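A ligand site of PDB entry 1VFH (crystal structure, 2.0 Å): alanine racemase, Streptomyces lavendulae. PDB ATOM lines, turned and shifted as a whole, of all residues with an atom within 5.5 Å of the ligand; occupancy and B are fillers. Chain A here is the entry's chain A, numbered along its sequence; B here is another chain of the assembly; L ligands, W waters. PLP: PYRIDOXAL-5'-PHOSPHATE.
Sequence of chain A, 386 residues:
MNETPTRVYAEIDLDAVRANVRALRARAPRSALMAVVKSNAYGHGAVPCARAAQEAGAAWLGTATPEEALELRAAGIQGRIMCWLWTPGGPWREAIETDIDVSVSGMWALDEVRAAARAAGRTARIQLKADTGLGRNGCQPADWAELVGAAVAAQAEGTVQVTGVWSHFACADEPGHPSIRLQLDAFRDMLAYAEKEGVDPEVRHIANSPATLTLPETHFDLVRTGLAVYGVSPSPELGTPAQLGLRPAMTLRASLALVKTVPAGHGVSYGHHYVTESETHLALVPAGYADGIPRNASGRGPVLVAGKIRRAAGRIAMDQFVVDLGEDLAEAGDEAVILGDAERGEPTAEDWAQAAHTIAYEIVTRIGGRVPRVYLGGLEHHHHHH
OG of Ser 209 lies within hydrogen-bond range of N of Gly 226 (3.3 Å). The side-chain hydroxyl (OG) of Ser 209 is in hydrogen-bond range of the backbone NH (N) of Ala 228, at 3.2 Å. A ring nitrogen (ND1) of His 168 is in hydrogen-bond range of the guanidinium group (NH2) of Arg 224 (3.1 Å). The backbone carbonyl oxygen (O) of Ala 207 lies within hydrogen-bond range of the backbone NH (N) of Arg 224 (3.0 Å). NE2 of His 168 sits at hydrogen-bond distance from OH of Tyr 270 of chain B, 3.0 Å away. The guanidinium group of Arg 136 is in salt-bridge range of OQ2 of KCX 129, at 2.8 Å. NH2 of Arg 136 is in hydrogen-bond range of OH of Tyr 270 of chain B. The backbone carbonyl oxygen (O) of Thr 225 lies within hydrogen-bond range of the backbone NH (N) of Val 36.
Water W2 lies within hydrogen-bond range of O3 of the ligand (2.7 Å), NE1 of Trp 84 (2.8 Å), OD1 of Asp 319 of chain B (2.9 Å) and NZ of Lys 38 (3.2 Å). Water W3 lies within hydrogen-bond range of O3P of the ligand (3.1 Å), ND2 of Asn 208 (3.2 Å) and OH of Tyr 270 of chain B (3.4 Å). Water W1 lies within hydrogen-bond range of the side-chain carboxylate (OD2) of Asp 319 of chain B (2.8 Å) and an oxygen (O3) of the ligand (3.5 Å).
C4A of the ligand is covalently linked to NZ of Lys 38 (1.5 Å). An oxygen (O2P) of the ligand lies within hydrogen-bond range of the side-chain hydroxyl of Tyr 42 (2.6 Å). An oxygen (O3P) of the ligand lies within hydrogen-bond range of the side-chain hydroxyl (OH) of Tyr 361 (2.6 Å). The backbone NH of Ser 209 is in hydrogen-bond range of an oxygen (O1P) of the ligand (2.9 Å). An oxygen (O1P) of the ligand lies within hydrogen-bond range of the side-chain hydroxyl (OG) of Ser 209 (2.6 Å). O1P of the ligand sits at hydrogen-bond distance from N of Gly 226. The backbone NH of Leu 227 is in hydrogen-bond range of an oxygen (O2P) of the ligand, 2.9 Å away. NE of Arg 224 is in hydrogen-bond range of N1 of the ligand (3.0 Å).
Residues that only touch the ligand: His 168 (3.4 Å), Arg 136 (3.6 Å), Trp 84 (3.6 Å), Pro 210 (3.6 Å), Trp 166 (3.6 Å), Asn 208 (3.8 Å), Thr 225 (3.8 Å) and Val 36 (3.9 Å). Hydrophobic or aromatic side chains within 4 Å of the ligand: Val 36, Tyr 42, Trp 84, Trp 166, His 168, Pro 210, Leu 227 and Tyr 361. Of the 22 residues printed, 15 come within 4 Å of the ligand.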
ATOM      1  N   VAL A  36      11.396  12.460  -6.409  1.00  0.00           N
ATOM      2  CA  VAL A  36      10.543  13.574  -6.042  1.00  0.00           C
ATOM      3  C   VAL A  36      10.532  14.607  -7.171  1.00  0.00           C
ATOM      4  O   VAL A  36      11.555  15.226  -7.481  1.00  0.00           O
ATOM      5  CB  VAL A  36      11.021  14.246  -4.756  1.00  0.00           C
ATOM      6  CG1 VAL A  36      10.061  15.362  -4.374  1.00  0.00           C
ATOM      7  CG2 VAL A  36      11.099  13.208  -3.632  1.00  0.00           C
ATOM      8  N   LYS A  38       8.281  17.268  -7.305  1.00  0.00           N
ATOM      9  CA  LYS A  38       7.475  18.400  -6.873  1.00  0.00           C
ATOM     10  C   LYS A  38       7.989  19.709  -7.495  1.00  0.00           C
ATOM     11  O   LYS A  38       9.152  19.810  -7.887  1.00  0.00           O
ATOM     12  CB  LYS A  38       7.506  18.515  -5.350  1.00  0.00           C
ATOM     13  CG  LYS A  38       8.861  18.859  -4.760  1.00  0.00           C
ATOM     14  CD  LYS A  38       8.716  19.661  -3.486  1.00  0.00           C
ATOM     15  CE  LYS A  38      10.019  19.747  -2.701  1.00  0.00           C
ATOM     16  NZ  LYS A  38      10.016  18.640  -1.732  1.00  0.00           N
ATOM     17  N   TYR A  42      11.373  20.409  -9.802  1.00  0.00           N
ATOM     18  CA  TYR A  42      12.401  21.378  -9.439  1.00  0.00           C
ATOM     19  C   TYR A  42      12.750  22.308 -10.613  1.00  0.00           C
ATOM     20  O   TYR A  42      13.905  22.718 -10.747  1.00  0.00           O
ATOM     21  CB  TYR A  42      13.652  20.626  -9.000  1.00  0.00           C
ATOM     22  CG  TYR A  42      13.535  19.974  -7.640  1.00  0.00           C
ATOM     23  CD1 TYR A  42      12.467  19.136  -7.354  1.00  0.00           C
ATOM     24  CD2 TYR A  42      14.492  20.186  -6.668  1.00  0.00           C
ATOM     25  CE1 TYR A  42      12.363  18.523  -6.110  1.00  0.00           C
ATOM     26  CE2 TYR A  42      14.405  19.577  -5.428  1.00  0.00           C
ATOM     27  CZ  TYR A  42      13.326  18.748  -5.152  1.00  0.00           C
ATOM     28  OH  TYR A  42      13.235  18.141  -3.924  1.00  0.00           O
ATOM     29  N   TRP A  84       2.176  14.750   0.017  1.00  0.00           N
ATOM     30  CA  TRP A  84       2.085  15.029   1.442  1.00  0.00           C
ATOM     31  C   TRP A  84       1.594  16.392   1.893  1.00  0.00           C
ATOM     32  O   TRP A  84       1.326  16.571   3.078  1.00  0.00           O
ATOM     33  CB  TRP A  84       3.464  14.804   2.054  1.00  0.00           C
ATOM     34  CG  TRP A  84       4.564  15.409   1.220  1.00  0.00           C
ATOM     35  CD1 TRP A  84       4.923  16.731   1.173  1.00  0.00           C
ATOM     36  CD2 TRP A  84       5.464  14.714   0.348  1.00  0.00           C
ATOM     37  NE1 TRP A  84       5.991  16.893   0.327  1.00  0.00           N
ATOM     38  CE2 TRP A  84       6.344  15.681  -0.197  1.00  0.00           C
ATOM     39  CE3 TRP A  84       5.616  13.370  -0.028  1.00  0.00           C
ATOM     40  CZ2 TRP A  84       7.366  15.334  -1.109  1.00  0.00           C
ATOM     41  CZ3 TRP A  84       6.623  13.036  -0.933  1.00  0.00           C
ATOM     42  CH2 TRP A  84       7.493  14.014  -1.458  1.00  0.00           C
ATOM     43  N   KCX A 129       2.836  10.473   8.966  1.00  0.00           N
ATOM     44  CA  KCX A 129       4.068  11.232   9.104  1.00  0.00           C
ATOM     45  CB  KCX A 129       4.069  12.500   8.242  1.00  0.00           C
ATOM     46  CG  KCX A 129       5.493  12.973   7.964  1.00  0.00           C
ATOM     47  CD  KCX A 129       5.607  14.483   7.791  1.00  0.00           C
ATOM     48  CE  KCX A 129       7.050  14.880   7.493  1.00  0.00           C
ATOM     49  NZ  KCX A 129       7.114  15.884   6.397  1.00  0.00           N
ATOM     50  C   KCX A 129       4.326  11.633  10.531  1.00  0.00           C
ATOM     51  O   KCX A 129       3.477  12.221  11.197  1.00  0.00           O
ATOM     52  CX  KCX A 129       7.316  17.306   6.593  1.00  0.00           C
ATOM     53  OQ1 KCX A 129       7.445  17.781   7.750  1.00  0.00           O
ATOM     54  OQ2 KCX A 129       7.315  18.079   5.611  1.00  0.00           O
ATOM     55  N   ARG A 136       7.937  20.943  11.124  1.00  0.00           N
ATOM     56  CA  ARG A 136       7.168  21.424   9.990  1.00  0.00           C
ATOM     57  C   ARG A 136       5.825  20.704   9.943  1.00  0.00           C
ATOM     58  O   ARG A 136       4.898  21.097  10.651  1.00  0.00           O
ATOM     59  CB  ARG A 136       7.937  21.171   8.689  1.00  0.00           C
ATOM     60  CG  ARG A 136       7.576  22.123   7.566  1.00  0.00           C
ATOM     61  CD  ARG A 136       8.618  22.074   6.469  1.00  0.00           C
ATOM     62  NE  ARG A 136       8.446  20.914   5.614  1.00  0.00           N
ATOM     63  CZ  ARG A 136       9.319  20.521   4.697  1.00  0.00           C
ATOM     64  NH1 ARG A 136       9.069  19.439   3.954  1.00  0.00           N
ATOM     65  NH2 ARG A 136      10.449  21.192   4.510  1.00  0.00           N
ATOM     66  N   TRP A 166       6.658   7.456   7.952  1.00  0.00           N
ATOM     67  CA  TRP A 166       7.819   8.229   7.530  1.00  0.00           C
ATOM     68  C   TRP A 166       8.022   9.545   8.258  1.00  0.00           C
ATOM     69  O   TRP A 166       7.153  10.012   9.002  1.00  0.00           O
ATOM     70  CB  TRP A 166       7.709   8.506   6.040  1.00  0.00           C
ATOM     71  CG  TRP A 166       6.551   9.399   5.701  1.00  0.00           C
ATOM     72  CD1 TRP A 166       5.217   9.137   5.898  1.00  0.00           C
ATOM     73  CD2 TRP A 166       6.619  10.708   5.120  1.00  0.00           C
ATOM     74  NE1 TRP A 166       4.461  10.204   5.475  1.00  0.00           N
ATOM     75  CE2 TRP A 166       5.285  11.187   4.994  1.00  0.00           C
ATOM     76  CE3 TRP A 166       7.674  11.540   4.694  1.00  0.00           C
ATOM     77  CZ2 TRP A 166       4.983  12.446   4.468  1.00  0.00           C
ATOM     78  CZ3 TRP A 166       7.372  12.799   4.168  1.00  0.00           C
ATOM     79  CH2 TRP A 166       6.041  13.229   4.054  1.00  0.00           C
ATOM     80  N   HIS A 168      10.938  13.343   8.077  1.00  0.00           N
ATOM     81  CA  HIS A 168      11.809  14.179   7.247  1.00  0.00           C
ATOM     82  C   HIS A 168      12.906  14.899   8.080  1.00  0.00           C
ATOM     83  O   HIS A 168      12.630  15.453   9.140  1.00  0.00           O
ATOM     84  CB  HIS A 168      10.925  15.201   6.514  1.00  0.00           C
ATOM     85  CG  HIS A 168      11.605  15.906   5.383  1.00  0.00           C
ATOM     86  ND1 HIS A 168      12.435  15.255   4.494  1.00  0.00           N
ATOM     87  CD2 HIS A 168      11.580  17.205   4.998  1.00  0.00           C
ATOM     88  CE1 HIS A 168      12.896  16.128   3.613  1.00  0.00           C
ATOM     89  NE2 HIS A 168      12.395  17.316   3.898  1.00  0.00           N
ATOM     90  N   ALA A 207      14.891   9.434   4.625  1.00  0.00           N
ATOM     91  CA  ALA A 207      15.957  10.104   3.895  1.00  0.00           C
ATOM     92  C   ALA A 207      15.579  10.921   2.667  1.00  0.00           C
ATOM     93  O   ALA A 207      14.706  10.536   1.884  1.00  0.00           O
ATOM     94  CB  ALA A 207      17.019   9.085   3.503  1.00  0.00           C
ATOM     95  N   ASN A 208      16.243  12.062   2.523  1.00  0.00           N
ATOM     96  CA  ASN A 208      16.064  12.951   1.389  1.00  0.00           C
ATOM     97  C   ASN A 208      17.371  12.782   0.606  1.00  0.00           C
ATOM     98  O   ASN A 208      18.109  11.827   0.855  1.00  0.00           O
ATOM     99  CB  ASN A 208      15.890  14.398   1.851  1.00  0.00           C
ATOM    100  CG  ASN A 208      16.936  14.828   2.850  1.00  0.00           C
ATOM    101  OD1 ASN A 208      17.810  14.046   3.230  1.00  0.00           O
ATOM    102  ND2 ASN A 208      16.863  16.085   3.291  1.00  0.00           N
ATOM    103  N   SER A 209      17.679  13.686  -0.324  1.00  0.00           N
ATOM    104  CA  SER A 209      18.904  13.553  -1.107  1.00  0.00           C
ATOM    105  C   SER A 209      20.202  13.561  -0.269  1.00  0.00           C
ATOM    106  O   SER A 209      21.030  12.665  -0.415  1.00  0.00           O
ATOM    107  CB  SER A 209      18.972  14.652  -2.170  1.00  0.00           C
ATOM    108  OG  SER A 209      18.251  14.279  -3.337  1.00  0.00           O
ATOM    109  N   PRO A 210      20.384  14.568   0.604  1.00  0.00           N
ATOM    110  CA  PRO A 210      21.621  14.561   1.404  1.00  0.00           C
ATOM    111  C   PRO A 210      21.809  13.343   2.320  1.00  0.00           C
ATOM    112  O   PRO A 210      22.907  12.830   2.445  1.00  0.00           O
ATOM    113  CB  PRO A 210      21.561  15.882   2.182  1.00  0.00           C
ATOM    114  CG  PRO A 210      20.129  16.284   2.158  1.00  0.00           C
ATOM    115  CD  PRO A 210      19.524  15.722   0.907  1.00  0.00           C
ATOM    116  N   ARG A 224      13.762   9.064  -0.559  1.00  0.00           N
ATOM    117  CA  ARG A 224      13.080  10.101  -1.323  1.00  0.00           C
ATOM    118  C   ARG A 224      14.117  11.078  -1.864  1.00  0.00           C
ATOM    119  O   ARG A 224      14.529  12.007  -1.181  1.00  0.00           O
ATOM    120  CB  ARG A 224      12.090  10.823  -0.420  1.00  0.00           C
ATOM    121  CG  ARG A 224      10.996   9.926   0.116  1.00  0.00           C
ATOM    122  CD  ARG A 224       9.968  10.716   0.923  1.00  0.00           C
ATOM    123  NE  ARG A 224      10.586  11.679   1.824  1.00  0.00           N
ATOM    124  CZ  ARG A 224      10.969  11.397   3.067  1.00  0.00           C
ATOM    125  NH1 ARG A 224      10.792  10.184   3.562  1.00  0.00           N
ATOM    126  NH2 ARG A 224      11.525  12.341   3.810  1.00  0.00           N
ATOM    127  N   THR A 225      14.535  10.873  -3.111  1.00  0.00           N
ATOM    128  CA  THR A 225      15.543  11.729  -3.720  1.00  0.00           C
ATOM    129  C   THR A 225      14.975  12.714  -4.728  1.00  0.00           C
ATOM    130  O   THR A 225      14.408  12.312  -5.756  1.00  0.00           O
ATOM    131  CB  THR A 225      16.624  10.894  -4.447  1.00  0.00           C
ATOM    132  OG1 THR A 225      16.000   9.985  -5.343  1.00  0.00           O
ATOM    133  CG2 THR A 225      17.472  10.132  -3.443  1.00  0.00           C
ATOM    134  N   GLY A 226      15.135  13.997  -4.435  1.00  0.00           N
ATOM    135  CA  GLY A 226      14.667  15.042  -5.316  1.00  0.00           C
ATOM    136  C   GLY A 226      15.824  15.695  -6.067  1.00  0.00           C
ATOM    137  O   GLY A 226      16.142  15.310  -7.195  1.00  0.00           O
ATOM    138  N   LEU A 227      16.488  16.650  -5.427  1.00  0.00           N
ATOM    139  CA  LEU A 227      17.579  17.389  -6.053  1.00  0.00           C
ATOM    140  C   LEU A 227      18.666  16.598  -6.764  1.00  0.00           C
ATOM    141  O   LEU A 227      18.962  16.885  -7.932  1.00  0.00           O
ATOM    142  CB  LEU A 227      18.247  18.332  -5.035  1.00  0.00           C
ATOM    143  CG  LEU A 227      19.155  19.393  -5.681  1.00  0.00           C
ATOM    144  CD1 LEU A 227      18.329  20.357  -6.516  1.00  0.00           C
ATOM    145  CD2 LEU A 227      19.920  20.135  -4.610  1.00  0.00           C
ATOM    146  N   ALA A 228      19.260  15.629  -6.075  1.00  0.00           N
ATOM    147  CA  ALA A 228      20.334  14.809  -6.662  1.00  0.00           C
ATOM    148  C   ALA A 228      19.959  14.203  -8.015  1.00  0.00           C
ATOM    149  O   ALA A 228      20.821  14.004  -8.883  1.00  0.00           O
ATOM    150  CB  ALA A 228      20.758  13.714  -5.674  1.00  0.00           C
ATOM    151  N   TYR A 361      19.061  24.764  -4.597  1.00  0.00           N
ATOM    152  CA  TYR A 361      17.665  24.352  -4.666  1.00  0.00           C
ATOM    153  C   TYR A 361      16.804  25.467  -5.260  1.00  0.00           C
ATOM    154  O   TYR A 361      16.022  25.231  -6.181  1.00  0.00           O
ATOM    155  CB  TYR A 361      17.135  24.024  -3.262  1.00  0.00           C
ATOM    156  CG  TYR A 361      17.506  22.667  -2.700  1.00  0.00           C
ATOM    157  CD1 TYR A 361      16.645  21.567  -2.815  1.00  0.00           C
ATOM    158  CD2 TYR A 361      18.695  22.498  -1.987  1.00  0.00           C
ATOM    159  CE1 TYR A 361      16.954  20.345  -2.224  1.00  0.00           C
ATOM    160  CE2 TYR A 361      19.010  21.279  -1.390  1.00  0.00           C
ATOM    161  CZ  TYR A 361      18.141  20.206  -1.512  1.00  0.00           C
ATOM    162  OH  TYR A 361      18.452  19.011  -0.908  1.00  0.00           O
ATOM    163  N   TYR B 270      14.444  23.632   8.265  1.00  0.00           N
ATOM    164  CA  TYR B 270      15.823  23.350   7.865  1.00  0.00           C
ATOM    165  C   TYR B 270      16.869  24.217   8.569  1.00  0.00           C
ATOM    166  O   TYR B 270      16.663  25.418   8.775  1.00  0.00           O
ATOM    167  CB  TYR B 270      15.987  23.528   6.354  1.00  0.00           C
ATOM    168  CG  TYR B 270      15.110  22.633   5.508  1.00  0.00           C
ATOM    169  CD1 TYR B 270      15.116  21.250   5.650  1.00  0.00           C
ATOM    170  CD2 TYR B 270      14.274  23.183   4.526  1.00  0.00           C
ATOM    171  CE1 TYR B 270      14.324  20.423   4.846  1.00  0.00           C
ATOM    172  CE2 TYR B 270      13.478  22.370   3.719  1.00  0.00           C
ATOM    173  CZ  TYR B 270      13.501  20.992   3.887  1.00  0.00           C
ATOM    174  OH  TYR B 270      12.712  20.183   3.086  1.00  0.00           O
ATOM    175  N   MET B 318      10.754  25.101   0.017  1.00  0.00           N
ATOM    176  CA  MET B 318      10.305  25.148  -1.359  1.00  0.00           C
ATOM    177  C   MET B 318       8.817  25.403  -1.516  1.00  0.00           C
ATOM    178  O   MET B 318       8.395  26.165  -2.384  1.00  0.00           O
ATOM    179  CB  MET B 318      10.705  23.864  -2.075  1.00  0.00           C
ATOM    180  CG  MET B 318      10.312  23.816  -3.544  1.00  0.00           C
ATOM    181  SD  MET B 318      11.093  22.487  -4.472  1.00  0.00           S
ATOM    182  CE  MET B 318      12.732  22.580  -3.854  1.00  0.00           C
ATOM    183  N   ASP B 319       8.012  24.768  -0.672  1.00  0.00           N
ATOM    184  CA  ASP B 319       6.559  24.906  -0.796  1.00  0.00           C
ATOM    185  C   ASP B 319       5.832  25.187   0.507  1.00  0.00           C
ATOM    186  O   ASP B 319       4.613  24.995   0.589  1.00  0.00           O
ATOM    187  CB  ASP B 319       5.975  23.647  -1.429  1.00  0.00           C
ATOM    188  CG  ASP B 319       6.773  22.401  -1.113  1.00  0.00           C
ATOM    189  OD1 ASP B 319       6.808  21.485  -1.954  1.00  0.00           O
ATOM    190  OD2 ASP B 319       7.388  22.340  -0.010  1.00  0.00           O
ATOM    191  N   GLN B 320       6.554  25.618   1.528  1.00  0.00           N
ATOM    192  CA  GLN B 320       5.910  25.898   2.792  1.00  0.00           C
ATOM    193  C   GLN B 320       6.875  26.509   3.782  1.00  0.00           C
ATOM    194  O   GLN B 320       8.087  26.478   3.575  1.00  0.00           O
ATOM    195  CB  GLN B 320       5.351  24.599   3.392  1.00  0.00           C
ATOM    196  CG  GLN B 320       6.428  23.592   3.790  1.00  0.00           C
ATOM    197  CD  GLN B 320       5.939  22.152   3.700  1.00  0.00           C
ATOM    198  OE1 GLN B 320       6.243  21.442   2.736  1.00  0.00           O
ATOM    199  NE2 GLN B 320       5.188  21.716   4.695  1.00  0.00           N
HETATM  200  N1  PLP L   1      10.986  14.590   1.290  1.00  0.00           N
HETATM  201  C2  PLP L   1      10.095  15.652   1.493  1.00  0.00           C
HETATM  202  C2A PLP L   1       9.034  15.603   2.561  1.00  0.00           C
HETATM  203  C3  PLP L   1      10.224  16.747   0.666  1.00  0.00           C
HETATM  204  O3  PLP L   1       9.415  17.817   0.810  1.00  0.00           O
HETATM  205  C4  PLP L   1      11.230  16.747  -0.330  1.00  0.00           C
HETATM  206  C4A PLP L   1      11.284  17.936  -1.386  1.00  0.00           C
HETATM  207  C5  PLP L   1      12.104  15.627  -0.450  1.00  0.00           C
HETATM  208  C6  PLP L   1      11.953  14.580   0.355  1.00  0.00           C
HETATM  209  C5A PLP L   1      13.258  15.596  -1.440  1.00  0.00           C
HETATM  210  O4P PLP L   1      14.339  16.389  -0.947  1.00  0.00           O
HETATM  211  P   PLP L   1      15.725  16.581  -1.703  1.00  0.00           P
HETATM  212  O1P PLP L   1      16.128  15.251  -2.161  1.00  0.00           O
HETATM  213  O2P PLP L   1      15.455  17.487  -2.816  1.00  0.00           O
HETATM  214  O3P PLP L   1      16.654  17.155  -0.749  1.00  0.00           O
HETATM  215  O   HOH W   1       9.822  21.279   0.951  1.00  0.00           O
HETATM  216  O   HOH W   2       7.371  19.334  -0.019  1.00  0.00           O
HETATM  217  O   HOH W   3      15.164  18.328   1.696  1.00  0.00           O
